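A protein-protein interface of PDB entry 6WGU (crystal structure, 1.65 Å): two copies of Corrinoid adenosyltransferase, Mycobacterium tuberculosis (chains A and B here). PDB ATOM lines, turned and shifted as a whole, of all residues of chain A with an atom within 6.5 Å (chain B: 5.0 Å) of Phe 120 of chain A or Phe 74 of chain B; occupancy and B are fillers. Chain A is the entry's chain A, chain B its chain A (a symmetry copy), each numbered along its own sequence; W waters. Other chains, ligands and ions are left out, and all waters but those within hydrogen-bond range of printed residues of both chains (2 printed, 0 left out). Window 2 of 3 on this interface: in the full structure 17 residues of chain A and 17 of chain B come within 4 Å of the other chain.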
ATOM      1  N   LEU A 117      16.508  21.164  20.846  1.00  0.00           N
ATOM      2  CA  LEU A 117      15.305  20.364  21.028  1.00  0.00           C
ATOM      3  C   LEU A 117      14.072  21.254  21.165  1.00  0.00           C
ATOM      4  O   LEU A 117      14.039  22.165  21.998  1.00  0.00           O
ATOM      5  CB  LEU A 117      15.441  19.476  22.264  1.00  0.00           C
ATOM      6  CG  LEU A 117      16.182  18.153  22.068  1.00  0.00           C
ATOM      7  CD1 LEU A 117      16.281  17.437  23.399  1.00  0.00           C
ATOM      8  CD2 LEU A 117      15.475  17.314  21.034  1.00  0.00           C
ATOM      9  N   LYS A 118      13.042  20.961  20.362  1.00  0.00           N
ATOM     10  CA  LYS A 118      11.781  21.688  20.454  1.00  0.00           C
ATOM     11  C   LYS A 118      10.897  21.119  21.557  1.00  0.00           C
ATOM     12  O   LYS A 118      10.263  21.879  22.298  1.00  0.00           O
ATOM     13  CB  LYS A 118      11.050  21.644  19.111  1.00  0.00           C
ATOM     14  N   SER A 119      10.857  19.793  21.693  1.00  0.00           N
ATOM     15  CA  SER A 119      10.132  19.137  22.769  1.00  0.00           C
ATOM     16  C   SER A 119      11.013  18.034  23.332  1.00  0.00           C
ATOM     17  O   SER A 119      12.163  17.836  22.907  1.00  0.00           O
ATOM     18  CB  SER A 119       8.779  18.568  22.305  1.00  0.00           C
ATOM     19  OG  SER A 119       8.048  17.974  23.393  1.00  0.00           O
ATOM     20  N   PHE A 120      10.459  17.314  24.298  1.00  0.00           N
ATOM     21  CA  PHE A 120      11.137  16.158  24.849  1.00  0.00           C
ATOM     22  C   PHE A 120      11.133  15.027  23.833  1.00  0.00           C
ATOM     23  O   PHE A 120      10.218  14.896  23.014  1.00  0.00           O
ATOM     24  CB  PHE A 120      10.470  15.696  26.143  1.00  0.00           C
ATOM     25  CG  PHE A 120      10.592  16.686  27.273  1.00  0.00           C
ATOM     26  CD1 PHE A 120       9.694  17.725  27.406  1.00  0.00           C
ATOM     27  CD2 PHE A 120      11.619  16.572  28.190  1.00  0.00           C
ATOM     28  CE1 PHE A 120       9.815  18.639  28.445  1.00  0.00           C
ATOM     29  CE2 PHE A 120      11.738  17.475  29.235  1.00  0.00           C
ATOM     30  CZ  PHE A 120      10.838  18.504  29.354  1.00  0.00           C
ATOM     31  N   VAL A 121      12.194  14.238  23.859  1.00  0.00           N
ATOM     32  CA  VAL A 121      12.393  13.163  22.900  1.00  0.00           C
ATOM     33  C   VAL A 121      11.832  11.863  23.463  1.00  0.00           C
ATOM     34  O   VAL A 121      12.072  11.523  24.628  1.00  0.00           O
ATOM     35  CB  VAL A 121      13.885  13.008  22.549  1.00  0.00           C
ATOM     36  CG1 VAL A 121      14.108  11.824  21.649  1.00  0.00           C
ATOM     37  CG2 VAL A 121      14.389  14.294  21.911  1.00  0.00           C
ATOM     38  N   LEU A 122      11.096  11.123  22.627  1.00  0.00           N
ATOM     39  CA  LEU A 122      10.732   9.750  22.940  1.00  0.00           C
ATOM     40  C   LEU A 122      11.703   8.787  22.274  1.00  0.00           C
ATOM     41  O   LEU A 122      12.213   9.058  21.180  1.00  0.00           O
ATOM     42  CB  LEU A 122       9.313   9.449  22.453  1.00  0.00           C
ATOM     43  CG  LEU A 122       8.233  10.331  23.040  1.00  0.00           C
ATOM     44  CD1 LEU A 122       6.859  10.003  22.457  1.00  0.00           C
ATOM     45  CD2 LEU A 122       8.198  10.239  24.549  1.00  0.00           C
ATOM     46  N   VAL A 185      11.561  11.457  17.480  1.00  0.00           N
ATOM     47  CA  VAL A 185      10.185  11.241  17.932  1.00  0.00           C
ATOM     48  C   VAL A 185       9.959  12.141  19.130  1.00  0.00           C
ATOM     49  O   VAL A 185      10.779  12.143  20.053  1.00  0.00           O
ATOM     50  CB  VAL A 185       9.948   9.768  18.309  1.00  0.00           C
ATOM     51  CG1 VAL A 185       8.489   9.562  18.723  1.00  0.00           C
ATOM     52  CG2 VAL A 185      10.300   8.857  17.134  1.00  0.00           C
ATOM     53  N   LEU A 186       8.898  12.943  19.102  1.00  0.00           N
ATOM     54  CA  LEU A 186       8.692  13.984  20.102  1.00  0.00           C
ATOM     55  C   LEU A 186       7.471  13.692  20.965  1.00  0.00           C
ATOM     56  O   LEU A 186       6.405  13.311  20.461  1.00  0.00           O
ATOM     57  CB  LEU A 186       8.519  15.356  19.439  1.00  0.00           C
ATOM     58  CG  LEU A 186       9.716  15.802  18.594  1.00  0.00           C
ATOM     59  CD1 LEU A 186       9.429  17.212  18.071  1.00  0.00           C
ATOM     60  CD2 LEU A 186      10.969  15.740  19.420  1.00  0.00           C
ATOM     61  N   TRP A 187       7.627  13.944  22.260  1.00  0.00           N
ATOM     62  CA  TRP A 187       6.510  13.918  23.189  1.00  0.00           C
ATOM     63  C   TRP A 187       5.546  15.064  22.911  1.00  0.00           C
ATOM     64  O   TRP A 187       5.949  16.180  22.559  1.00  0.00           O
ATOM     65  CB  TRP A 187       7.031  14.016  24.630  1.00  0.00           C
ATOM     66  CG  TRP A 187       5.959  14.065  25.689  1.00  0.00           C
ATOM     67  CD1 TRP A 187       5.174  13.029  26.114  1.00  0.00           C
ATOM     68  CD2 TRP A 187       5.586  15.200  26.471  1.00  0.00           C
ATOM     69  NE1 TRP A 187       4.317  13.462  27.103  1.00  0.00           N
ATOM     70  CE2 TRP A 187       4.557  14.788  27.343  1.00  0.00           C
ATOM     71  CE3 TRP A 187       6.018  16.531  26.516  1.00  0.00           C
ATOM     72  CZ2 TRP A 187       3.949  15.656  28.235  1.00  0.00           C
ATOM     73  CZ3 TRP A 187       5.418  17.395  27.410  1.00  0.00           C
ATOM     74  CH2 TRP A 187       4.391  16.959  28.257  1.00  0.00           C
ATOM     75  N   ARG A 188       4.264  14.796  23.102  1.00  0.00           N
ATOM     76  CA  ARG A 188       3.242  15.810  22.964  1.00  0.00           C
ATOM     77  C   ARG A 188       2.488  15.986  24.276  1.00  0.00           C
ATOM     78  O   ARG A 188       1.971  14.999  24.821  1.00  0.00           O
ATOM     79  CB  ARG A 188       2.254  15.425  21.855  1.00  0.00           C
ATOM     80  CG  ARG A 188       2.877  15.262  20.487  1.00  0.00           C
ATOM     81  CD  ARG A 188       1.780  15.029  19.459  1.00  0.00           C
ATOM     82  NE  ARG A 188       2.289  14.544  18.179  1.00  0.00           N
ATOM     83  CZ  ARG A 188       1.522  14.038  17.217  1.00  0.00           C
ATOM     84  NH1 ARG A 188       0.209  13.948  17.388  1.00  0.00           N
ATOM     85  NH2 ARG A 188       2.068  13.616  16.085  1.00  0.00           N
ATOM     86  N   ASN B  46       9.919   2.104  27.489  1.00  0.00           N
ATOM     87  CA  ASN B  46       9.640   2.964  26.350  1.00  0.00           C
ATOM     88  C   ASN B  46      10.620   2.713  25.215  1.00  0.00           C
ATOM     89  O   ASN B  46      10.217   2.662  24.049  1.00  0.00           O
ATOM     90  CB  ASN B  46       9.693   4.419  26.808  1.00  0.00           C
ATOM     91  CG  ASN B  46       8.792   5.336  26.008  1.00  0.00           C
ATOM     92  OD1 ASN B  46       8.259   4.980  24.959  1.00  0.00           O
ATOM     93  ND2 ASN B  46       8.618   6.540  26.511  1.00  0.00           N
ATOM     94  N   ILE B  69       1.228   4.866  23.370  1.00  0.00           N
ATOM     95  CA  ILE B  69       1.814   4.257  24.558  1.00  0.00           C
ATOM     96  C   ILE B  69       3.150   4.913  24.902  1.00  0.00           C
ATOM     97  O   ILE B  69       3.446   5.147  26.074  1.00  0.00           O
ATOM     98  CB  ILE B  69       1.932   2.737  24.344  1.00  0.00           C
ATOM     99  CG1 ILE B  69       0.518   2.121  24.296  1.00  0.00           C
ATOM    100  CG2 ILE B  69       2.743   2.108  25.431  1.00  0.00           C
ATOM    101  CD1 ILE B  69       0.478   0.725  23.779  1.00  0.00           C
ATOM    102  N   GLN B  70       3.998   5.176  23.911  1.00  0.00           N
ATOM    103  CA  GLN B  70       5.253   5.849  24.229  1.00  0.00           C
ATOM    104  C   GLN B  70       5.010   7.197  24.884  1.00  0.00           C
ATOM    105  O   GLN B  70       5.749   7.601  25.790  1.00  0.00           O
ATOM    106  CB  GLN B  70       6.088   6.039  22.975  1.00  0.00           C
ATOM    107  CG  GLN B  70       6.627   4.728  22.432  1.00  0.00           C
ATOM    108  CD  GLN B  70       7.804   4.977  21.522  1.00  0.00           C
ATOM    109  OE1 GLN B  70       7.653   5.445  20.371  1.00  0.00           O
ATOM    110  NE2 GLN B  70       9.001   4.720  22.040  1.00  0.00           N
ATOM    111  N   ASN B  71       4.025   7.942  24.387  1.00  0.00           N
ATOM    112  CA  ASN B  71       3.684   9.216  25.001  1.00  0.00           C
ATOM    113  C   ASN B  71       3.232   9.019  26.443  1.00  0.00           C
ATOM    114  O   ASN B  71       3.664   9.758  27.338  1.00  0.00           O
ATOM    115  CB  ASN B  71       2.609   9.909  24.163  1.00  0.00           C
ATOM    116  CG  ASN B  71       2.767  11.382  24.165  1.00  0.00           C
ATOM    117  OD1 ASN B  71       3.549  11.943  23.379  1.00  0.00           O
ATOM    118  ND2 ASN B  71       2.004  12.056  25.034  1.00  0.00           N
ATOM    119  N   ASP B  72       2.390   8.003  26.686  1.00  0.00           N
ATOM    120  CA  ASP B  72       1.927   7.678  28.031  1.00  0.00           C
ATOM    121  C   ASP B  72       3.079   7.289  28.953  1.00  0.00           C
ATOM    122  O   ASP B  72       3.063   7.624  30.140  1.00  0.00           O
ATOM    123  CB  ASP B  72       0.947   6.501  27.992  1.00  0.00           C
ATOM    124  CG  ASP B  72      -0.320   6.777  27.207  1.00  0.00           C
ATOM    125  OD1 ASP B  72      -0.636   7.962  26.884  1.00  0.00           O
ATOM    126  OD2 ASP B  72      -1.047   5.764  26.938  1.00  0.00           O
ATOM    127  N   LEU B  73       4.045   6.506  28.454  1.00  0.00           N
ATOM    128  CA  LEU B  73       5.134   6.061  29.317  1.00  0.00           C
ATOM    129  C   LEU B  73       6.019   7.222  29.732  1.00  0.00           C
ATOM    130  O   LEU B  73       6.625   7.179  30.809  1.00  0.00           O
ATOM    131  CB  LEU B  73       5.972   4.994  28.621  1.00  0.00           C
ATOM    132  CG  LEU B  73       5.252   3.644  28.503  1.00  0.00           C
ATOM    133  CD1 LEU B  73       6.094   2.691  27.611  1.00  0.00           C
ATOM    134  CD2 LEU B  73       5.106   2.967  29.889  1.00  0.00           C
ATOM    135  N   PHE B  74       6.147   8.242  28.881  1.00  0.00           N
ATOM    136  CA  PHE B  74       6.821   9.467  29.299  1.00  0.00           C
ATOM    137  C   PHE B  74       6.075  10.091  30.466  1.00  0.00           C
ATOM    138  O   PHE B  74       6.678  10.502  31.475  1.00  0.00           O
ATOM    139  CB  PHE B  74       6.922  10.440  28.118  1.00  0.00           C
ATOM    140  CG  PHE B  74       7.601  11.725  28.443  1.00  0.00           C
ATOM    141  CD1 PHE B  74       6.897  12.767  29.017  1.00  0.00           C
ATOM    142  CD2 PHE B  74       8.944  11.896  28.172  1.00  0.00           C
ATOM    143  CE1 PHE B  74       7.521  13.948  29.337  1.00  0.00           C
ATOM    144  CE2 PHE B  74       9.580  13.093  28.471  1.00  0.00           C
ATOM    145  CZ  PHE B  74       8.869  14.117  29.056  1.00  0.00           C
ATOM    146  N   ASP B  75       4.749  10.191  30.327  1.00  0.00           N
ATOM    147  CA  ASP B  75       3.926  10.739  31.400  1.00  0.00           C
ATOM    148  C   ASP B  75       4.052   9.894  32.669  1.00  0.00           C
ATOM    149  O   ASP B  75       4.094  10.427  33.793  1.00  0.00           O
ATOM    150  CB  ASP B  75       2.459  10.787  30.967  1.00  0.00           C
ATOM    151  CG  ASP B  75       2.195  11.680  29.765  1.00  0.00           C
ATOM    152  OD1 ASP B  75       3.098  12.427  29.296  1.00  0.00           O
ATOM    153  OD2 ASP B  75       1.029  11.657  29.272  1.00  0.00           O
ATOM    154  N   ALA B  76       4.095   8.565  32.509  1.00  0.00           N
ATOM    155  CA  ALA B  76       4.194   7.697  33.675  1.00  0.00           C
ATOM    156  C   ALA B  76       5.514   7.911  34.399  1.00  0.00           C
ATOM    157  O   ALA B  76       5.548   7.936  35.632  1.00  0.00           O
ATOM    158  CB  ALA B  76       4.038   6.228  33.272  1.00  0.00           C
ATOM    159  N   GLY B  77       6.617   8.045  33.654  1.00  0.00           N
ATOM    160  CA  GLY B  77       7.894   8.306  34.290  1.00  0.00           C
ATOM    161  C   GLY B  77       7.898   9.634  35.019  1.00  0.00           C
ATOM    162  O   GLY B  77       8.414   9.734  36.131  1.00  0.00           O
ATOM    163  N   ALA B  78       7.343  10.676  34.391  1.00  0.00           N
ATOM    164  CA  ALA B  78       7.242  11.978  35.043  1.00  0.00           C
ATOM    165  C   ALA B  78       6.428  11.888  36.325  1.00  0.00           C
ATOM    166  O   ALA B  78       6.773  12.507  37.340  1.00  0.00           O
ATOM    167  CB  ALA B  78       6.610  12.986  34.079  1.00  0.00           C
ATOM    168  N   LEU B  93       1.229  16.532  35.723  1.00  0.00           N
ATOM    169  CA  LEU B  93       1.597  15.553  34.697  1.00  0.00           C
ATOM    170  C   LEU B  93       1.497  14.191  35.392  1.00  0.00           C
ATOM    171  O   LEU B  93       2.464  13.695  35.972  1.00  0.00           O
ATOM    172  CB  LEU B  93       2.972  15.811  34.118  1.00  0.00           C
ATOM    173  CG  LEU B  93       3.330  14.846  32.974  1.00  0.00           C
ATOM    174  CD1 LEU B  93       2.231  14.792  31.914  1.00  0.00           C
ATOM    175  CD2 LEU B  93       4.656  15.220  32.322  1.00  0.00           C
HETATM  176  O   HOH W   1       0.830  13.966  27.761  1.00  0.00           O
HETATM  177  O   HOH W   2       4.206  11.656  20.678  1.00  0.00           O
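NE1 of Trp 187 of chain A lies close to ND2 of Asn 71 of chain B.
NE1 of Trp 187 of chain A is in hydrogen-bond range of OD1 of Asp 75 of chain B (2.7 Å).
The backbone carbonyl oxygen (O) of Arg 188 of chain A sits at hydrogen-bond distance from the side-chain amide nitrogen (ND2) of Asn 71 of chain B (3.0 Å).
OG of Ser 119 of chain A sits at hydrogen-bond distance from O of Trp 187 of chain A, at 2.9 Å.
O of Phe 120 of chain A lies within hydrogen-bond range of N of Trp 187 of chain A, 2.9 Å away.
The backbone NH (N) of Leu 122 of chain A is in hydrogen-bond range of the backbone carbonyl oxygen (O) of Val 185 of chain A (2.8 Å).
NE2 of Gln 70 of chain B sits close to OD1 of Asn 46 of chain B (3.0 Å).
Phe 120 of chain A touches Phe 74 of chain B.
Gln 70 of chain B touches Leu 122 of chain A (O to CD2, 3.8 Å).
CD1 of Leu 122 of chain A touches OD1 of Asn 71 of chain B, at 3.9 Å.
Leu 122 of chain A touches Phe 74 of chain B.
Phe 74 of chain B touches Trp 187 of chain A (CD1 to NE1, 3.3 Å).
Printed residues of chain B within 4 Å of Phe 120 of chain A: Phe 74.
Of chain A, only Phe 120, Leu 122 and Trp 187 come within 4 Å of Phe 74 of chain B.
Printed residues of chain B within 4 Å of Leu 122 of chain A: Gln 70, Asn 71 and Phe 74.
Of the printed residues of chain A, Asp 75 of chain B touches Trp 187.
Of the printed residues of chain A, Asn 71 of chain B touches Leu 122 (3.9 Å), Trp 187 (3.4 Å) and Arg 188 (3.0 Å).
Printed residues of chain A within 4 Å of Gln 70 of chain B: Leu 122 (3.8 Å).
Of the printed residues of chain B, Arg 188 of chain A touches Asn 71.
Leu 186 of chain A touches none of the printed residues of chain B.
Ile 69 of chain B touches none of the printed residues of chain A.
The nearest residue of chain A that does not touch Phe 74 of chain B is Val 121 of chain A (4.7 Å).
The nearest printed residue of chain B that does not touch Leu 122 of chain A is Asn 46 of chain B (4.2 Å).
Of the 10 printed residues of chain A, 4 touch a printed residue of chain B.
Hydrophobic or aromatic side chains of chain A within 4 Å of the printed part of chain B: Phe 120, Leu 122 and Trp 187.
Among the printed residues, 8 pairs touch across the chains.
Among the printed residues, no Asp or Glu carboxylate lies within 4 Å of a Lys or Arg side-chain nitrogen of the other chain.
No position is printed for both chains.
Of the 8 pairs that touch across the chains among the printed residues, none has its exchanged pair printed and touching as well.
Water W2 bridges the backbone carbonyl oxygen (O) of Leu 186 of chain A (2.8 Å) and the side-chain amide oxygen (OD1) of Asn 71 of chain B (2.8 Å).
Water W1 bridges OD2 of Asp 75 of chain B (2.8 Å) and O of Arg 188 of chain A (3.3 Å).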
